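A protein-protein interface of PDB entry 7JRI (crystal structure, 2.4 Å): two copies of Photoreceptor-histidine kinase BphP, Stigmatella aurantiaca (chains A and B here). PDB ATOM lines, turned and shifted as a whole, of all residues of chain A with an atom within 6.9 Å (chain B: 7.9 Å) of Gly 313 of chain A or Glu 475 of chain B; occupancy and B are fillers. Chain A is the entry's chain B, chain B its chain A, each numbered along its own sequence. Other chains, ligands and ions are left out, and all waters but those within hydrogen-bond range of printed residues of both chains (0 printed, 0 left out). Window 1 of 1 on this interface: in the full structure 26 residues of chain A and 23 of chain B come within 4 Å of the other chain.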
ATOM      1  N   ARG A 308      -1.558  18.799  -2.755  1.00  0.00           N
ATOM      2  CA  ARG A 308      -2.459  18.717  -3.934  1.00  0.00           C
ATOM      3  C   ARG A 308      -2.487  17.271  -4.480  1.00  0.00           C
ATOM      4  O   ARG A 308      -3.596  16.725  -4.713  1.00  0.00           O
ATOM      5  CB  ARG A 308      -2.010  19.733  -4.992  1.00  0.00           C
ATOM      6  CG  ARG A 308      -2.245  21.200  -4.634  1.00  0.00           C
ATOM      7  CD  ARG A 308      -3.583  21.724  -5.126  1.00  0.00           C
ATOM      8  NE  ARG A 308      -3.770  23.172  -5.117  1.00  0.00           N
ATOM      9  CZ  ARG A 308      -4.267  23.882  -4.107  1.00  0.00           C
ATOM     10  NH1 ARG A 308      -4.610  23.299  -2.973  1.00  0.00           N
ATOM     11  NH2 ARG A 308      -4.412  25.188  -4.232  1.00  0.00           N
ATOM     12  N   ALA A 309      -1.314  16.664  -4.690  1.00  0.00           N
ATOM     13  CA  ALA A 309      -1.154  15.369  -5.391  1.00  0.00           C
ATOM     14  C   ALA A 309      -1.613  14.207  -4.502  1.00  0.00           C
ATOM     15  O   ALA A 309      -2.044  13.187  -5.084  1.00  0.00           O
ATOM     16  CB  ALA A 309       0.274  15.186  -5.844  1.00  0.00           C
ATOM     17  N   ALA A 310      -1.536  14.348  -3.170  1.00  0.00           N
ATOM     18  CA  ALA A 310      -2.048  13.363  -2.181  1.00  0.00           C
ATOM     19  C   ALA A 310      -3.575  13.341  -2.224  1.00  0.00           C
ATOM     20  O   ALA A 310      -4.134  12.260  -1.915  1.00  0.00           O
ATOM     21  CB  ALA A 310      -1.567  13.655  -0.780  1.00  0.00           C
ATOM     22  N   LEU A 311      -4.208  14.482  -2.564  1.00  0.00           N
ATOM     23  CA  LEU A 311      -5.649  14.526  -2.955  1.00  0.00           C
ATOM     24  C   LEU A 311      -5.807  13.599  -4.173  1.00  0.00           C
ATOM     25  O   LEU A 311      -6.435  12.528  -4.032  1.00  0.00           O
ATOM     26  CB  LEU A 311      -6.124  15.964  -3.248  1.00  0.00           C
ATOM     27  CG  LEU A 311      -6.698  16.782  -2.081  1.00  0.00           C
ATOM     28  CD1 LEU A 311      -7.903  16.108  -1.427  1.00  0.00           C
ATOM     29  CD2 LEU A 311      -5.639  17.080  -1.031  1.00  0.00           C
ATOM     30  N   LEU A 312      -5.169  13.935  -5.294  1.00  0.00           N
ATOM     31  CA  LEU A 312      -5.338  13.213  -6.587  1.00  0.00           C
ATOM     32  C   LEU A 312      -4.954  11.727  -6.482  1.00  0.00           C
ATOM     33  O   LEU A 312      -5.535  10.934  -7.243  1.00  0.00           O
ATOM     34  CB  LEU A 312      -4.538  13.936  -7.675  1.00  0.00           C
ATOM     35  CG  LEU A 312      -5.375  14.891  -8.521  1.00  0.00           C
ATOM     36  CD1 LEU A 312      -5.914  16.036  -7.671  1.00  0.00           C
ATOM     37  CD2 LEU A 312      -4.573  15.409  -9.708  1.00  0.00           C
ATOM     38  N   GLY A 313      -4.040  11.355  -5.576  1.00  0.00           N
ATOM     39  CA  GLY A 313      -3.705   9.947  -5.255  1.00  0.00           C
ATOM     40  C   GLY A 313      -4.805   9.229  -4.472  1.00  0.00           C
ATOM     41  O   GLY A 313      -5.029   8.045  -4.726  1.00  0.00           O
ATOM     42  N   GLN A 314      -5.427   9.886  -3.492  1.00  0.00           N
ATOM     43  CA  GLN A 314      -6.704   9.423  -2.884  1.00  0.00           C
ATOM     44  C   GLN A 314      -7.684   9.136  -4.024  1.00  0.00           C
ATOM     45  O   GLN A 314      -7.972   7.969  -4.284  1.00  0.00           O
ATOM     46  CB  GLN A 314      -7.337  10.494  -1.976  1.00  0.00           C
ATOM     47  CG  GLN A 314      -7.343  10.182  -0.487  1.00  0.00           C
ATOM     48  CD  GLN A 314      -6.106  10.680   0.211  1.00  0.00           C
ATOM     49  OE1 GLN A 314      -4.999  10.209  -0.042  1.00  0.00           O
ATOM     50  NE2 GLN A 314      -6.298  11.617   1.121  1.00  0.00           N
ATOM     51  N   LEU A 315      -8.075  10.209  -4.715  1.00  0.00           N
ATOM     52  CA  LEU A 315      -9.196  10.347  -5.684  1.00  0.00           C
ATOM     53  C   LEU A 315      -9.135   9.301  -6.805  1.00  0.00           C
ATOM     54  O   LEU A 315     -10.129   9.258  -7.569  1.00  0.00           O
ATOM     55  CB  LEU A 315      -9.085  11.760  -6.271  1.00  0.00           C
ATOM     56  CG  LEU A 315     -10.366  12.371  -6.832  1.00  0.00           C
ATOM     57  CD1 LEU A 315     -11.113  13.147  -5.752  1.00  0.00           C
ATOM     58  CD2 LEU A 315     -10.044  13.272  -8.020  1.00  0.00           C
ATOM     59  N   ALA A 316      -8.029   8.537  -6.926  1.00  0.00           N
ATOM     60  CA  ALA A 316      -7.681   7.679  -8.093  1.00  0.00           C
ATOM     61  C   ALA A 316      -7.633   6.181  -7.746  1.00  0.00           C
ATOM     62  O   ALA A 316      -7.760   5.359  -8.686  1.00  0.00           O
ATOM     63  CB  ALA A 316      -6.350   8.104  -8.658  1.00  0.00           C
ATOM     64  N   THR A 317      -7.386   5.830  -6.476  1.00  0.00           N
ATOM     65  CA  THR A 317      -7.350   4.428  -5.980  1.00  0.00           C
ATOM     66  C   THR A 317      -8.775   4.001  -5.600  1.00  0.00           C
ATOM     67  O   THR A 317      -9.252   2.984  -6.142  1.00  0.00           O
ATOM     68  CB  THR A 317      -6.275   4.258  -4.898  1.00  0.00           C
ATOM     69  OG1 THR A 317      -5.776   5.530  -4.492  1.00  0.00           O
ATOM     70  CG2 THR A 317      -5.101   3.453  -5.404  1.00  0.00           C
ATOM     71  N   ALA A 318      -9.459   4.763  -4.746  1.00  0.00           N
ATOM     72  CA  ALA A 318     -10.931   4.692  -4.612  1.00  0.00           C
ATOM     73  C   ALA A 318     -11.546   4.529  -6.009  1.00  0.00           C
ATOM     74  O   ALA A 318     -12.412   3.655  -6.177  1.00  0.00           O
ATOM     75  CB  ALA A 318     -11.454   5.923  -3.923  1.00  0.00           C
ATOM     76  N   LEU B 312       2.162  15.372 -20.804  1.00  0.00           N
ATOM     77  CA  LEU B 312       1.000  14.539 -20.365  1.00  0.00           C
ATOM     78  C   LEU B 312      -0.334  15.161 -20.810  1.00  0.00           C
ATOM     79  O   LEU B 312      -1.316  14.405 -20.972  1.00  0.00           O
ATOM     80  CB  LEU B 312       1.043  14.428 -18.839  1.00  0.00           C
ATOM     81  CG  LEU B 312       0.505  13.122 -18.258  1.00  0.00           C
ATOM     82  CD1 LEU B 312       0.992  12.896 -16.827  1.00  0.00           C
ATOM     83  CD2 LEU B 312      -1.017  13.085 -18.328  1.00  0.00           C
ATOM     84  N   GLN B 378       3.379  -0.273  -2.135  1.00  0.00           N
ATOM     85  CA  GLN B 378       1.912   0.009  -2.250  1.00  0.00           C
ATOM     86  C   GLN B 378       1.559   0.431  -3.672  1.00  0.00           C
ATOM     87  O   GLN B 378       0.365   0.461  -3.975  1.00  0.00           O
ATOM     88  CB  GLN B 378       1.370   1.212  -1.450  1.00  0.00           C
ATOM     89  CG  GLN B 378       1.954   1.477  -0.070  1.00  0.00           C
ATOM     90  CD  GLN B 378       3.177   2.376  -0.061  1.00  0.00           C
ATOM     91  OE1 GLN B 378       3.510   3.050  -1.033  1.00  0.00           O
ATOM     92  NE2 GLN B 378       3.885   2.331   1.058  1.00  0.00           N
ATOM     93  N   THR B 379       2.542   0.888  -4.446  1.00  0.00           N
ATOM     94  CA  THR B 379       2.342   1.858  -5.552  1.00  0.00           C
ATOM     95  C   THR B 379       3.572   2.011  -6.457  1.00  0.00           C
ATOM     96  O   THR B 379       3.439   2.721  -7.470  1.00  0.00           O
ATOM     97  CB  THR B 379       2.037   3.233  -4.950  1.00  0.00           C
ATOM     98  OG1 THR B 379       3.029   3.482  -3.947  1.00  0.00           O
ATOM     99  CG2 THR B 379       0.661   3.325  -4.326  1.00  0.00           C
ATOM    100  N   SER B 380       4.742   1.476  -6.086  1.00  0.00           N
ATOM    101  CA  SER B 380       6.052   1.886  -6.663  1.00  0.00           C
ATOM    102  C   SER B 380       7.179   0.951  -6.218  1.00  0.00           C
ATOM    103  O   SER B 380       7.106   0.386  -5.109  1.00  0.00           O
ATOM    104  CB  SER B 380       6.356   3.284  -6.234  1.00  0.00           C
ATOM    105  OG  SER B 380       6.400   3.358  -4.810  1.00  0.00           O
ATOM    106  N   ALA B 405       7.795   0.324 -10.936  1.00  0.00           N
ATOM    107  CA  ALA B 405       6.472  -0.254 -10.633  1.00  0.00           C
ATOM    108  C   ALA B 405       5.427   0.853 -10.544  1.00  0.00           C
ATOM    109  O   ALA B 405       5.802   2.000 -10.285  1.00  0.00           O
ATOM    110  CB  ALA B 405       6.522  -1.024  -9.337  1.00  0.00           C
ATOM    111  N   VAL B 406       4.161   0.453 -10.711  1.00  0.00           N
ATOM    112  CA  VAL B 406       2.904   1.202 -10.408  1.00  0.00           C
ATOM    113  C   VAL B 406       1.789   0.156 -10.471  1.00  0.00           C
ATOM    114  O   VAL B 406       1.881  -0.699 -11.376  1.00  0.00           O
ATOM    115  CB  VAL B 406       2.653   2.351 -11.407  1.00  0.00           C
ATOM    116  CG1 VAL B 406       3.552   3.553 -11.170  1.00  0.00           C
ATOM    117  CG2 VAL B 406       2.780   1.867 -12.843  1.00  0.00           C
ATOM    118  N   ARG B 407       0.819   0.203  -9.548  1.00  0.00           N
ATOM    119  CA  ARG B 407      -0.249  -0.820  -9.399  1.00  0.00           C
ATOM    120  C   ARG B 407      -1.581  -0.234  -9.882  1.00  0.00           C
ATOM    121  O   ARG B 407      -2.098   0.680  -9.225  1.00  0.00           O
ATOM    122  CB  ARG B 407      -0.360  -1.272  -7.942  1.00  0.00           C
ATOM    123  CG  ARG B 407       0.969  -1.374  -7.202  1.00  0.00           C
ATOM    124  CD  ARG B 407       0.865  -2.131  -5.883  1.00  0.00           C
ATOM    125  NE  ARG B 407       0.145  -3.384  -6.031  1.00  0.00           N
ATOM    126  CZ  ARG B 407       0.288  -4.462  -5.271  1.00  0.00           C
ATOM    127  NH1 ARG B 407       1.142  -4.482  -4.259  1.00  0.00           N
ATOM    128  NH2 ARG B 407      -0.427  -5.539  -5.544  1.00  0.00           N
ATOM    129  N   TRP B 418       8.588   0.565 -17.042  1.00  0.00           N
ATOM    130  CA  TRP B 418       9.577   1.221 -17.956  1.00  0.00           C
ATOM    131  C   TRP B 418      11.018   0.860 -17.531  1.00  0.00           C
ATOM    132  O   TRP B 418      11.555   1.595 -16.681  1.00  0.00           O
ATOM    133  CB  TRP B 418       9.471   2.762 -17.967  1.00  0.00           C
ATOM    134  CG  TRP B 418       8.122   3.396 -17.846  1.00  0.00           C
ATOM    135  CD1 TRP B 418       7.521   4.208 -18.761  1.00  0.00           C
ATOM    136  CD2 TRP B 418       7.238   3.371 -16.714  1.00  0.00           C
ATOM    137  NE1 TRP B 418       6.293   4.626 -18.307  1.00  0.00           N
ATOM    138  CE2 TRP B 418       6.098   4.135 -17.048  1.00  0.00           C
ATOM    139  CE3 TRP B 418       7.274   2.744 -15.471  1.00  0.00           C
ATOM    140  CZ2 TRP B 418       5.023   4.297 -16.181  1.00  0.00           C
ATOM    141  CZ3 TRP B 418       6.210   2.904 -14.613  1.00  0.00           C
ATOM    142  CH2 TRP B 418       5.102   3.670 -14.966  1.00  0.00           C
ATOM    143  N   ASP B 470       9.748  12.943 -12.659  1.00  0.00           N
ATOM    144  CA  ASP B 470      10.114  11.727 -13.424  1.00  0.00           C
ATOM    145  C   ASP B 470       9.475  10.613 -12.605  1.00  0.00           C
ATOM    146  O   ASP B 470       8.276  10.411 -12.704  1.00  0.00           O
ATOM    147  CB  ASP B 470      11.640  11.727 -13.638  1.00  0.00           C
ATOM    148  CG  ASP B 470      12.326  10.436 -14.043  1.00  0.00           C
ATOM    149  OD1 ASP B 470      11.998   9.982 -15.125  1.00  0.00           O
ATOM    150  OD2 ASP B 470      13.234   9.946 -13.287  1.00  0.00           O
ATOM    151  N   LEU B 471      10.217  10.041 -11.684  1.00  0.00           N
ATOM    152  CA  LEU B 471       9.627   9.476 -10.445  1.00  0.00           C
ATOM    153  C   LEU B 471       8.185  10.001 -10.282  1.00  0.00           C
ATOM    154  O   LEU B 471       7.290   9.205 -10.401  1.00  0.00           O
ATOM    155  CB  LEU B 471      10.551   9.871  -9.285  1.00  0.00           C
ATOM    156  CG  LEU B 471      10.439   9.070  -7.997  1.00  0.00           C
ATOM    157  CD1 LEU B 471      10.205  10.004  -6.823  1.00  0.00           C
ATOM    158  CD2 LEU B 471       9.336   8.011  -8.083  1.00  0.00           C
ATOM    159  N   GLY B 472       7.963  11.302 -10.094  1.00  0.00           N
ATOM    160  CA  GLY B 472       6.636  11.902  -9.796  1.00  0.00           C
ATOM    161  C   GLY B 472       5.580  11.762 -10.906  1.00  0.00           C
ATOM    162  O   GLY B 472       4.353  11.674 -10.578  1.00  0.00           O
ATOM    163  N   ALA B 473       5.996  11.764 -12.172  1.00  0.00           N
ATOM    164  CA  ALA B 473       5.132  11.449 -13.337  1.00  0.00           C
ATOM    165  C   ALA B 473       4.787   9.951 -13.367  1.00  0.00           C
ATOM    166  O   ALA B 473       4.951   9.336 -14.411  1.00  0.00           O
ATOM    167  CB  ALA B 473       5.816  11.873 -14.623  1.00  0.00           C
ATOM    168  N   ALA B 474       4.294   9.387 -12.268  1.00  0.00           N
ATOM    169  CA  ALA B 474       3.912   7.962 -12.177  1.00  0.00           C
ATOM    170  C   ALA B 474       2.546   7.845 -11.500  1.00  0.00           C
ATOM    171  O   ALA B 474       1.612   7.322 -12.153  1.00  0.00           O
ATOM    172  CB  ALA B 474       4.982   7.214 -11.440  1.00  0.00           C
ATOM    173  N   GLU B 475       2.425   8.359 -10.267  1.00  0.00           N
ATOM    174  CA  GLU B 475       1.146   8.465  -9.521  1.00  0.00           C
ATOM    175  C   GLU B 475       0.044   9.057 -10.406  1.00  0.00           C
ATOM    176  O   GLU B 475      -1.120   8.938 -10.019  1.00  0.00           O
ATOM    177  CB  GLU B 475       1.310   9.364  -8.297  1.00  0.00           C
ATOM    178  CG  GLU B 475       0.105   9.338  -7.385  1.00  0.00           C
ATOM    179  CD  GLU B 475      -0.441   7.930  -7.229  1.00  0.00           C
ATOM    180  OE1 GLU B 475      -1.688   7.772  -7.042  1.00  0.00           O
ATOM    181  OE2 GLU B 475       0.393   6.983  -7.300  1.00  0.00           O
ATOM    182  N   GLY B 476       0.405   9.748 -11.497  1.00  0.00           N
ATOM    183  CA  GLY B 476      -0.543  10.419 -12.408  1.00  0.00           C
ATOM    184  C   GLY B 476      -0.976   9.448 -13.488  1.00  0.00           C
ATOM    185  O   GLY B 476      -2.139   8.980 -13.468  1.00  0.00           O
ATOM    186  N   PHE B 477      -0.030   9.090 -14.350  1.00  0.00           N
ATOM    187  CA  PHE B 477      -0.182   8.083 -15.429  1.00  0.00           C
ATOM    188  C   PHE B 477      -1.118   6.968 -14.943  1.00  0.00           C
ATOM    189  O   PHE B 477      -2.019   6.539 -15.689  1.00  0.00           O
ATOM    190  CB  PHE B 477       1.196   7.545 -15.827  1.00  0.00           C
ATOM    191  CG  PHE B 477       1.179   6.797 -17.129  1.00  0.00           C
ATOM    192  CD1 PHE B 477       0.830   5.457 -17.173  1.00  0.00           C
ATOM    193  CD2 PHE B 477       1.425   7.459 -18.319  1.00  0.00           C
ATOM    194  CE1 PHE B 477       0.779   4.782 -18.378  1.00  0.00           C
ATOM    195  CE2 PHE B 477       1.353   6.785 -19.529  1.00  0.00           C
ATOM    196  CZ  PHE B 477       1.039   5.443 -19.554  1.00  0.00           C
ATOM    197  N   ARG B 478      -0.895   6.535 -13.699  1.00  0.00           N
ATOM    198  CA  ARG B 478      -1.628   5.443 -13.002  1.00  0.00           C
ATOM    199  C   ARG B 478      -3.068   5.905 -12.745  1.00  0.00           C
ATOM    200  O   ARG B 478      -3.956   5.102 -12.958  1.00  0.00           O
ATOM    201  CB  ARG B 478      -0.809   5.009 -11.776  1.00  0.00           C
ATOM    202  CG  ARG B 478      -1.598   4.441 -10.609  1.00  0.00           C
ATOM    203  CD  ARG B 478      -1.848   5.531  -9.596  1.00  0.00           C
ATOM    204  NE  ARG B 478      -2.300   5.074  -8.288  1.00  0.00           N
ATOM    205  CZ  ARG B 478      -1.578   4.379  -7.427  1.00  0.00           C
ATOM    206  NH1 ARG B 478      -0.351   3.993  -7.718  1.00  0.00           N
ATOM    207  NH2 ARG B 478      -2.100   4.058  -6.263  1.00  0.00           N
ATOM    208  N   GLY B 479      -3.275   7.167 -12.363  1.00  0.00           N
ATOM    209  CA  GLY B 479      -4.612   7.760 -12.133  1.00  0.00           C
ATOM    210  C   GLY B 479      -5.382   7.991 -13.428  1.00  0.00           C
ATOM    211  O   GLY B 479      -6.605   7.742 -13.455  1.00  0.00           O
ATOM    212  N   ALA B 480      -4.675   8.431 -14.468  1.00  0.00           N
ATOM    213  CA  ALA B 480      -5.222   8.801 -15.796  1.00  0.00           C
ATOM    214  C   ALA B 480      -5.118   7.616 -16.770  1.00  0.00           C
ATOM    215  O   ALA B 480      -5.122   7.868 -17.995  1.00  0.00           O
ATOM    216  CB  ALA B 480      -4.488  10.022 -16.315  1.00  0.00           C
ATOM    217  N   LEU B 481      -5.016   6.388 -16.255  1.00  0.00           N
ATOM    218  CA  LEU B 481      -5.282   5.140 -17.026  1.00  0.00           C
ATOM    219  C   LEU B 481      -6.711   4.678 -16.724  1.00  0.00           C
ATOM    220  O   LEU B 481      -7.218   4.936 -15.620  1.00  0.00           O
ATOM    221  CB  LEU B 481      -4.247   4.048 -16.702  1.00  0.00           C
ATOM    222  CG  LEU B 481      -3.179   3.841 -17.781  1.00  0.00           C
ATOM    223  CD1 LEU B 481      -2.174   2.788 -17.363  1.00  0.00           C
ATOM    224  CD2 LEU B 481      -3.808   3.465 -19.118  1.00  0.00           C
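Of the 20 printed residues of chain B, 3 touch a printed residue of chain A.
Printed residues of chain B that touch a printed residue of chain A: Glu 475, Arg 478 and Gly 479.
Of the 11 printed residues of chain A, 3 touch a printed residue of chain B.
Printed residues of chain A that touch a printed residue of chain B: Gly 313, Ala 316 and Thr 317.
Hydrophobic or aromatic side chains of chain A that line the printed part of chain B: Ala 316.
Among the printed residues, 3 pairs touch across the chains.
Among the printed residues, no Asp or Glu carboxylate lies within 4 Å of a Lys or Arg side-chain nitrogen of the other chain.
Of chain B, only Glu 475 comes within 4 Å of Gly 313 of chain A.
Of the printed residues of chain B, Ala 316 of chain A touches Gly 479 (3.9 Å).
Of the printed residues of chain B, Thr 317 of chain A touches Arg 478 (3.2 Å).
Of the printed residues of chain A, Glu 475 of chain B touches Gly 313.
Printed residues of chain A within 4 Å of Arg 478 of chain B: Thr 317.
Printed residues of chain A within 4 Å of Gly 479 of chain B: Ala 316 (3.9 Å).
The nearest printed residue of chain A that does not touch Glu 475 of chain B is Ala 316 of chain A (4.9 Å).
The nearest printed residue of chain A that does not touch Gly 479 of chain B is Leu 312 of chain A (5.9 Å).
Glu 475 of chain B touches Gly 313 of chain A.
CB of Ala 316 of chain A touches CA of Gly 479 of chain B, 3.9 Å away.
Arg 478 of chain B touches Thr 317 of chain A.
The backbone carbonyl oxygen (O) of Gln 314 of chain A sits at hydrogen-bond distance from the side-chain hydroxyl (OG1) of Thr 317 of chain A (3.3 Å).
The side-chain hydroxyl (OG1) of Thr 317 of chain A is in hydrogen-bond range of the backbone carbonyl oxygen (O) of Gly 313 of chain A (2.6 Å).
NE of Arg 478 of chain B lies within salt-bridge range of OE1 of Glu 475 of chain B, at 3.0 Å.
Position printed for both chains: 312.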
